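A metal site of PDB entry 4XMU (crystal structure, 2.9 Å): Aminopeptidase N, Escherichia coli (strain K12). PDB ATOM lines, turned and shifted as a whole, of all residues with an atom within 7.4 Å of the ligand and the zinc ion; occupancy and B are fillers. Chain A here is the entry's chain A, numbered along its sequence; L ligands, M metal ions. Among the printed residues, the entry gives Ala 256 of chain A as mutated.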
ATOM      1  N   GLN A 115       3.602 -25.113  -5.771  1.00  0.00           N
ATOM      2  CA  GLN A 115       3.510 -24.067  -6.758  1.00  0.00           C
ATOM      3  C   GLN A 115       2.681 -22.927  -6.229  1.00  0.00           C
ATOM      4  O   GLN A 115       1.489 -23.073  -5.995  1.00  0.00           O
ATOM      5  CB  GLN A 115       2.911 -24.571  -8.065  1.00  0.00           C
ATOM      6  CG  GLN A 115       2.961 -23.559  -9.179  1.00  0.00           C
ATOM      7  CD  GLN A 115       4.348 -22.950  -9.371  1.00  0.00           C
ATOM      8  OE1 GLN A 115       5.401 -23.604  -9.105  1.00  0.00           O
ATOM      9  NE2 GLN A 115       4.371 -21.686  -9.769  1.00  0.00           N
ATOM     10  N   GLU A 117       3.268 -19.402  -7.601  1.00  0.00           N
ATOM     11  CA  GLU A 117       3.028 -18.337  -8.596  1.00  0.00           C
ATOM     12  C   GLU A 117       1.745 -18.667  -9.328  1.00  0.00           C
ATOM     13  O   GLU A 117       1.644 -19.785  -9.771  1.00  0.00           O
ATOM     14  CB  GLU A 117       4.185 -18.153  -9.611  1.00  0.00           C
ATOM     15  CG  GLU A 117       3.929 -16.950 -10.516  1.00  0.00           C
ATOM     16  CD  GLU A 117       5.110 -16.469 -11.313  1.00  0.00           C
ATOM     17  OE1 GLU A 117       5.997 -17.261 -11.642  1.00  0.00           O
ATOM     18  OE2 GLU A 117       5.116 -15.271 -11.666  1.00  0.00           O
ATOM     19  N   TYR A 181       4.949 -15.557  -3.548  1.00  0.00           N
ATOM     20  CA  TYR A 181       4.934 -16.402  -4.789  1.00  0.00           C
ATOM     21  C   TYR A 181       6.231 -17.202  -5.075  1.00  0.00           C
ATOM     22  O   TYR A 181       6.240 -18.125  -5.889  1.00  0.00           O
ATOM     23  CB  TYR A 181       4.518 -15.628  -6.047  1.00  0.00           C
ATOM     24  CG  TYR A 181       5.567 -14.753  -6.713  1.00  0.00           C
ATOM     25  CD1 TYR A 181       6.460 -15.284  -7.639  1.00  0.00           C
ATOM     26  CD2 TYR A 181       5.641 -13.398  -6.470  1.00  0.00           C
ATOM     27  CE1 TYR A 181       7.408 -14.479  -8.274  1.00  0.00           C
ATOM     28  CE2 TYR A 181       6.575 -12.592  -7.106  1.00  0.00           C
ATOM     29  CZ  TYR A 181       7.465 -13.131  -8.000  1.00  0.00           C
ATOM     30  OH  TYR A 181       8.409 -12.368  -8.632  1.00  0.00           O
ATOM     31  N   LEU A 182       7.304 -16.802  -4.407  1.00  0.00           N
ATOM     32  CA  LEU A 182       8.605 -17.343  -4.550  1.00  0.00           C
ATOM     33  C   LEU A 182       8.952 -18.322  -3.452  1.00  0.00           C
ATOM     34  O   LEU A 182      10.042 -18.876  -3.466  1.00  0.00           O
ATOM     35  CB  LEU A 182       9.625 -16.201  -4.528  1.00  0.00           C
ATOM     36  CG  LEU A 182       9.695 -15.327  -5.797  1.00  0.00           C
ATOM     37  CD1 LEU A 182      10.772 -14.241  -5.668  1.00  0.00           C
ATOM     38  CD2 LEU A 182       9.980 -16.172  -7.045  1.00  0.00           C
ATOM     39  N   PHE A 254       3.229 -31.080 -12.870  1.00  0.00           N
ATOM     40  CA  PHE A 254       3.556 -29.663 -12.878  1.00  0.00           C
ATOM     41  C   PHE A 254       2.783 -29.039 -14.028  1.00  0.00           C
ATOM     42  O   PHE A 254       2.765 -29.576 -15.140  1.00  0.00           O
ATOM     43  CB  PHE A 254       5.063 -29.454 -13.063  1.00  0.00           C
ATOM     44  CG  PHE A 254       5.558 -28.161 -12.530  1.00  0.00           C
ATOM     45  CD1 PHE A 254       5.633 -27.947 -11.142  1.00  0.00           C
ATOM     46  CD2 PHE A 254       5.957 -27.146 -13.375  1.00  0.00           C
ATOM     47  CE1 PHE A 254       6.070 -26.737 -10.609  1.00  0.00           C
ATOM     48  CE2 PHE A 254       6.388 -25.934 -12.854  1.00  0.00           C
ATOM     49  CZ  PHE A 254       6.455 -25.731 -11.464  1.00  0.00           C
ATOM     50  N   ALA A 256       3.181 -25.534 -15.102  1.00  0.00           N
ATOM     51  CA  ALA A 256       4.075 -24.701 -15.921  1.00  0.00           C
ATOM     52  C   ALA A 256       5.190 -25.578 -16.525  1.00  0.00           C
ATOM     53  O   ALA A 256       5.083 -26.804 -16.571  1.00  0.00           O
ATOM     54  CB  ALA A 256       4.643 -23.569 -15.050  1.00  0.00           C
ATOM     55  N   GLY A 257       6.234 -24.923 -17.022  1.00  0.00           N
ATOM     56  CA  GLY A 257       7.465 -25.602 -17.426  1.00  0.00           C
ATOM     57  C   GLY A 257       8.447 -25.659 -16.289  1.00  0.00           C
ATOM     58  O   GLY A 257       9.102 -26.675 -16.090  1.00  0.00           O
ATOM     59  N   ALA A 258       8.539 -24.551 -15.552  1.00  0.00           N
ATOM     60  CA  ALA A 258       9.443 -24.448 -14.436  1.00  0.00           C
ATOM     61  C   ALA A 258       9.176 -23.155 -13.623  1.00  0.00           C
ATOM     62  O   ALA A 258       8.479 -22.258 -14.063  1.00  0.00           O
ATOM     63  CB  ALA A 258      10.876 -24.487 -14.950  1.00  0.00           C
ATOM     64  N   MET A 259       9.751 -23.086 -12.427  1.00  0.00           N
ATOM     65  CA  MET A 259       9.514 -21.987 -11.497  1.00  0.00           C
ATOM     66  C   MET A 259      10.792 -21.465 -10.760  1.00  0.00           C
ATOM     67  O   MET A 259      11.456 -22.171 -10.043  1.00  0.00           O
ATOM     68  CB  MET A 259       8.421 -22.430 -10.508  1.00  0.00           C
ATOM     69  CG  MET A 259       7.957 -21.358  -9.530  1.00  0.00           C
ATOM     70  SD  MET A 259       7.335 -19.897 -10.377  1.00  0.00           S
ATOM     71  CE  MET A 259       7.679 -18.603  -9.190  1.00  0.00           C
ATOM     72  N   GLU A 260      11.105 -20.201 -11.035  1.00  0.00           N
ATOM     73  CA  GLU A 260      12.190 -19.450 -10.397  1.00  0.00           C
ATOM     74  C   GLU A 260      12.118 -19.249  -8.871  1.00  0.00           C
ATOM     75  O   GLU A 260      12.565 -18.244  -8.338  1.00  0.00           O
ATOM     76  CB  GLU A 260      12.326 -18.073 -11.092  1.00  0.00           C
ATOM     77  CG  GLU A 260      11.165 -17.095 -10.886  1.00  0.00           C
ATOM     78  CD  GLU A 260       9.928 -17.397 -11.706  1.00  0.00           C
ATOM     79  OE1 GLU A 260       9.785 -18.527 -12.178  1.00  0.00           O
ATOM     80  OE2 GLU A 260       9.079 -16.525 -11.874  1.00  0.00           O
ATOM     81  N   VAL A 290      15.104 -23.260 -20.733  1.00  0.00           N
ATOM     82  CA  VAL A 290      14.266 -23.140 -19.527  1.00  0.00           C
ATOM     83  C   VAL A 290      15.123 -23.027 -18.238  1.00  0.00           C
ATOM     84  O   VAL A 290      14.851 -22.155 -17.401  1.00  0.00           O
ATOM     85  CB  VAL A 290      13.200 -24.246 -19.459  1.00  0.00           C
ATOM     86  CG1 VAL A 290      12.400 -24.178 -18.160  1.00  0.00           C
ATOM     87  CG2 VAL A 290      12.287 -24.129 -20.667  1.00  0.00           C
ATOM     88  N   HIS A 293      16.498 -19.588 -18.316  1.00  0.00           N
ATOM     89  CA  HIS A 293      15.365 -18.709 -18.017  1.00  0.00           C
ATOM     90  C   HIS A 293      15.155 -18.634 -16.515  1.00  0.00           C
ATOM     91  O   HIS A 293      15.185 -17.524 -15.984  1.00  0.00           O
ATOM     92  CB  HIS A 293      14.076 -19.184 -18.743  1.00  0.00           C
ATOM     93  CG  HIS A 293      12.891 -18.266 -18.565  1.00  0.00           C
ATOM     94  ND1 HIS A 293      12.522 -17.339 -19.525  1.00  0.00           N
ATOM     95  CD2 HIS A 293      12.005 -18.124 -17.546  1.00  0.00           C
ATOM     96  CE1 HIS A 293      11.481 -16.661 -19.093  1.00  0.00           C
ATOM     97  NE2 HIS A 293      11.148 -17.106 -17.894  1.00  0.00           N
ATOM     98  N   GLU A 294      14.942 -19.766 -15.820  1.00  0.00           N
ATOM     99  CA  GLU A 294      14.674 -19.691 -14.393  1.00  0.00           C
ATOM    100  C   GLU A 294      15.852 -19.118 -13.680  1.00  0.00           C
ATOM    101  O   GLU A 294      15.682 -18.329 -12.792  1.00  0.00           O
ATOM    102  CB  GLU A 294      14.326 -21.033 -13.766  1.00  0.00           C
ATOM    103  CG  GLU A 294      13.120 -21.782 -14.316  1.00  0.00           C
ATOM    104  CD  GLU A 294      11.961 -20.897 -14.784  1.00  0.00           C
ATOM    105  OE1 GLU A 294      11.641 -19.861 -14.146  1.00  0.00           O
ATOM    106  OE2 GLU A 294      11.377 -21.248 -15.825  1.00  0.00           O
ATOM    107  N   HIS A 297      15.898 -15.256 -13.933  1.00  0.00           N
ATOM    108  CA  HIS A 297      14.915 -14.729 -12.958  1.00  0.00           C
ATOM    109  C   HIS A 297      15.491 -14.360 -11.612  1.00  0.00           C
ATOM    110  O   HIS A 297      14.905 -13.535 -10.918  1.00  0.00           O
ATOM    111  CB  HIS A 297      13.735 -15.700 -12.740  1.00  0.00           C
ATOM    112  CG  HIS A 297      12.582 -15.469 -13.662  1.00  0.00           C
ATOM    113  ND1 HIS A 297      12.073 -14.205 -13.904  1.00  0.00           N
ATOM    114  CD2 HIS A 297      11.828 -16.326 -14.392  1.00  0.00           C
ATOM    115  CE1 HIS A 297      11.048 -14.291 -14.732  1.00  0.00           C
ATOM    116  NE2 HIS A 297      10.887 -15.562 -15.050  1.00  0.00           N
ATOM    117  N   THR A 300      16.164 -10.655 -12.512  1.00  0.00           N
ATOM    118  CA  THR A 300      15.045 -10.056 -13.180  1.00  0.00           C
ATOM    119  C   THR A 300      13.811 -10.875 -12.813  1.00  0.00           C
ATOM    120  O   THR A 300      13.309 -11.692 -13.617  1.00  0.00           O
ATOM    121  CB  THR A 300      15.285 -10.035 -14.675  1.00  0.00           C
ATOM    122  OG1 THR A 300      15.558 -11.357 -15.141  1.00  0.00           O
ATOM    123  CG2 THR A 300      16.488  -9.130 -15.001  1.00  0.00           C
ATOM    124  N   TRP A 309       0.526  -7.981 -10.153  1.00  0.00           N
ATOM    125  CA  TRP A 309       0.539  -8.941 -11.251  1.00  0.00           C
ATOM    126  C   TRP A 309       0.324  -8.345 -12.643  1.00  0.00           C
ATOM    127  O   TRP A 309       0.609  -8.987 -13.651  1.00  0.00           O
ATOM    128  CB  TRP A 309      -0.407 -10.107 -10.964  1.00  0.00           C
ATOM    129  CG  TRP A 309       0.099 -10.972  -9.863  1.00  0.00           C
ATOM    130  CD1 TRP A 309      -0.485 -11.224  -8.685  1.00  0.00           C
ATOM    131  CD2 TRP A 309       1.345 -11.670  -9.843  1.00  0.00           C
ATOM    132  NE1 TRP A 309       0.308 -12.033  -7.916  1.00  0.00           N
ATOM    133  CE2 TRP A 309       1.440 -12.326  -8.615  1.00  0.00           C
ATOM    134  CE3 TRP A 309       2.416 -11.792 -10.749  1.00  0.00           C
ATOM    135  CZ2 TRP A 309       2.532 -13.097  -8.257  1.00  0.00           C
ATOM    136  CZ3 TRP A 309       3.511 -12.549 -10.407  1.00  0.00           C
ATOM    137  CH2 TRP A 309       3.569 -13.204  -9.169  1.00  0.00           C
ATOM    138  N   LEU A 312       3.558  -8.271 -14.769  1.00  0.00           N
ATOM    139  CA  LEU A 312       4.195  -9.563 -15.007  1.00  0.00           C
ATOM    140  C   LEU A 312       5.258  -9.440 -16.090  1.00  0.00           C
ATOM    141  O   LEU A 312       6.337  -9.997 -15.948  1.00  0.00           O
ATOM    142  CB  LEU A 312       3.181 -10.646 -15.402  1.00  0.00           C
ATOM    143  CG  LEU A 312       3.720 -12.072 -15.558  1.00  0.00           C
ATOM    144  CD1 LEU A 312       4.308 -12.582 -14.274  1.00  0.00           C
ATOM    145  CD2 LEU A 312       2.599 -13.001 -15.944  1.00  0.00           C
ATOM    146  N   LYS A 315       9.182  -8.778 -15.326  1.00  0.00           N
ATOM    147  CA  LYS A 315      10.054  -9.932 -15.145  1.00  0.00           C
ATOM    148  C   LYS A 315      10.087 -10.929 -16.351  1.00  0.00           C
ATOM    149  O   LYS A 315      11.163 -11.406 -16.725  1.00  0.00           O
ATOM    150  CB  LYS A 315       9.745 -10.646 -13.829  1.00  0.00           C
ATOM    151  CG  LYS A 315       8.412 -11.367 -13.725  1.00  0.00           C
ATOM    152  CD  LYS A 315       8.312 -11.988 -12.337  1.00  0.00           C
ATOM    153  CE  LYS A 315       7.138 -12.947 -12.080  1.00  0.00           C
ATOM    154  NZ  LYS A 315       7.273 -14.292 -12.721  1.00  0.00           N
ATOM    155  N   GLU A 316       8.942 -11.222 -16.978  1.00  0.00           N
ATOM    156  CA  GLU A 316       8.873 -12.251 -18.015  1.00  0.00           C
ATOM    157  C   GLU A 316       9.378 -11.797 -19.403  1.00  0.00           C
ATOM    158  O   GLU A 316      10.057 -12.551 -20.116  1.00  0.00           O
ATOM    159  CB  GLU A 316       7.453 -12.797 -18.145  1.00  0.00           C
ATOM    160  CG  GLU A 316       6.931 -13.507 -16.925  1.00  0.00           C
ATOM    161  CD  GLU A 316       7.773 -14.700 -16.491  1.00  0.00           C
ATOM    162  OE1 GLU A 316       8.695 -15.162 -17.247  1.00  0.00           O
ATOM    163  OE2 GLU A 316       7.515 -15.172 -15.371  1.00  0.00           O
ATOM    164  N   GLY A 317       8.998 -10.591 -19.809  1.00  0.00           N
ATOM    165  CA  GLY A 317       9.479 -10.076 -21.083  1.00  0.00           C
ATOM    166  C   GLY A 317      10.981  -9.889 -21.047  1.00  0.00           C
ATOM    167  O   GLY A 317      11.695 -10.221 -22.003  1.00  0.00           O
ATOM    168  N   THR A 319      13.009 -11.454 -18.813  1.00  0.00           N
ATOM    169  CA  THR A 319      13.666 -12.756 -18.606  1.00  0.00           C
ATOM    170  C   THR A 319      13.644 -13.637 -19.881  1.00  0.00           C
ATOM    171  O   THR A 319      14.571 -14.388 -20.128  1.00  0.00           O
ATOM    172  CB  THR A 319      13.114 -13.476 -17.373  1.00  0.00           C
ATOM    173  OG1 THR A 319      13.352 -12.672 -16.211  1.00  0.00           O
ATOM    174  CG2 THR A 319      13.794 -14.769 -17.168  1.00  0.00           C
ATOM    175  N   VAL A 320      12.581 -13.554 -20.676  1.00  0.00           N
ATOM    176  CA  VAL A 320      12.522 -14.237 -21.985  1.00  0.00           C
ATOM    177  C   VAL A 320      13.603 -13.626 -22.899  1.00  0.00           C
ATOM    178  O   VAL A 320      14.403 -14.360 -23.509  1.00  0.00           O
ATOM    179  CB  VAL A 320      11.093 -14.133 -22.621  1.00  0.00           C
ATOM    180  CG1 VAL A 320      11.080 -14.448 -24.099  1.00  0.00           C
ATOM    181  CG2 VAL A 320      10.122 -15.033 -21.885  1.00  0.00           C
ATOM    182  N   ASP A 323      16.725 -15.200 -21.920  1.00  0.00           N
ATOM    183  CA  ASP A 323      16.917 -16.582 -22.411  1.00  0.00           C
ATOM    184  C   ASP A 323      17.157 -16.668 -23.945  1.00  0.00           C
ATOM    185  O   ASP A 323      17.749 -17.630 -24.425  1.00  0.00           O
ATOM    186  CB  ASP A 323      15.819 -17.556 -21.877  1.00  0.00           C
ATOM    187  CG  ASP A 323      14.542 -17.613 -22.733  1.00  0.00           C
ATOM    188  OD1 ASP A 323      14.581 -17.791 -23.980  1.00  0.00           O
ATOM    189  OD2 ASP A 323      13.453 -17.548 -22.117  1.00  0.00           O
ATOM    190  N   TYR A 372      -0.382 -15.663 -18.312  1.00  0.00           N
ATOM    191  CA  TYR A 372       0.958 -16.222 -18.609  1.00  0.00           C
ATOM    192  C   TYR A 372       0.913 -16.642 -20.062  1.00  0.00           C
ATOM    193  O   TYR A 372       0.696 -17.827 -20.381  1.00  0.00           O
ATOM    194  CB  TYR A 372       1.329 -17.390 -17.683  1.00  0.00           C
ATOM    195  CG  TYR A 372       1.624 -16.874 -16.295  1.00  0.00           C
ATOM    196  CD1 TYR A 372       0.593 -16.566 -15.422  1.00  0.00           C
ATOM    197  CD2 TYR A 372       2.932 -16.614 -15.883  1.00  0.00           C
ATOM    198  CE1 TYR A 372       0.857 -16.039 -14.175  1.00  0.00           C
ATOM    199  CE2 TYR A 372       3.200 -16.106 -14.625  1.00  0.00           C
ATOM    200  CZ  TYR A 372       2.141 -15.828 -13.782  1.00  0.00           C
ATOM    201  OH  TYR A 372       2.363 -15.302 -12.555  1.00  0.00           O
ATOM    202  N   TYR A 377       4.924 -12.937 -22.407  1.00  0.00           N
ATOM    203  CA  TYR A 377       6.262 -13.514 -22.508  1.00  0.00           C
ATOM    204  C   TYR A 377       6.987 -13.012 -23.742  1.00  0.00           C
ATOM    205  O   TYR A 377       7.957 -12.285 -23.659  1.00  0.00           O
ATOM    206  CB  TYR A 377       6.203 -15.056 -22.525  1.00  0.00           C
ATOM    207  CG  TYR A 377       6.087 -15.644 -21.164  1.00  0.00           C
ATOM    208  CD1 TYR A 377       5.035 -15.301 -20.331  1.00  0.00           C
ATOM    209  CD2 TYR A 377       7.060 -16.501 -20.660  1.00  0.00           C
ATOM    210  CE1 TYR A 377       4.945 -15.820 -19.053  1.00  0.00           C
ATOM    211  CE2 TYR A 377       6.977 -17.042 -19.387  1.00  0.00           C
ATOM    212  CZ  TYR A 377       5.913 -16.689 -18.587  1.00  0.00           C
ATOM    213  OH  TYR A 377       5.755 -17.184 -17.312  1.00  0.00           O
HETATM  214  N1  LIG L   1       7.614 -17.460 -13.894  1.00  0.00           N
HETATM  215  C1  LIG L   1       7.657 -18.881 -14.335  1.00  0.00           C
HETATM  216  C2  LIG L   1       8.312 -18.943 -15.691  1.00  0.00           C
HETATM  217  O1  LIG L   1       7.955 -18.238 -16.601  1.00  0.00           O
HETATM  218  C3  LIG L   1       6.248 -19.464 -14.390  1.00  0.00           C
HETATM  219  O2  LIG L   1       9.227 -19.675 -15.938  1.00  0.00           O
HETATM  220 ZN    ZN M   1       9.723 -16.644 -16.342  1.00  0.00          ZN
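Of the 25 residues printed, 3 come within 4 Å of the zinc ion.
Along chain A the residues within 4 Å of the zinc ion span positions 293 to 316.
The zinc ion is bound by OE1 of Glu 316, at 2.0 Å.
NE2 of His 297 is bound to the zinc ion (2.0 Å).
NE2 of His 293 binds the zinc ion.
The zinc ion is bound by O1 of the ligand (2.4 Å).
The zinc ion has four donor atoms within binding distance.
Slightly farther from the zinc ion lies the side-chain carboxylate (OE2) of Glu 316 (2.8 Å).
OE1 of Glu 294 is in hydrogen-bond range of N of Glu 260 (3.2 Å).
The side-chain carboxylate (OE2) of Glu 260 is in salt-bridge range of the side-chain amino group (NZ) of Lys 315 (3.0 Å).
The side-chain carboxylate of Glu 316 is in hydrogen-bond range of the side-chain hydroxyl of Tyr 377, at 3.3 Å.
The side-chain carboxylate of Glu 117 lies within hydrogen-bond range of the side-chain hydroxyl of Tyr 372.
ND1 of His 293 is in hydrogen-bond range of OD2 of Asp 323 (2.8 Å).
OE2 of Glu 117 lies within salt-bridge range of NZ of Lys 315 (2.6 Å).
The backbone carbonyl oxygen of Thr 300 lies within hydrogen-bond range of a ring nitrogen (ND1) of His 297 (2.8 Å).
The side-chain amide nitrogen (NE2) of Gln 115 is in hydrogen-bond range of the backbone carbonyl oxygen (O) of Glu 117.
The side-chain carboxylate (OE2) of Glu 260 is in salt-bridge range of a nitrogen (N1) of the ligand (2.7 Å).
The side-chain carboxylate of Glu 117 is in salt-bridge range of a nitrogen (N1) of the ligand (2.8 Å).
A nitrogen (N1) of the ligand sits close to the side-chain amino group (NZ) of Lys 315 (3.4 Å).
The side-chain hydroxyl (OH) of Tyr 377 sits close to an oxygen (O1) of the ligand.
The side-chain carboxylate (OE2) of Glu 294 sits close to an oxygen (O2) of the ligand, 2.7 Å away.
O2 of the ligand lies close to O of Ala 258, at 3.3 Å.
Hydrophobic or aromatic side chains that line the ligand: His 293 and Tyr 377.
Within 4 Å of the ligand: Glu 117, Ala 258, Glu 260, His 293, Glu 294, His 297, Lys 315, Glu 316 and Tyr 377.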
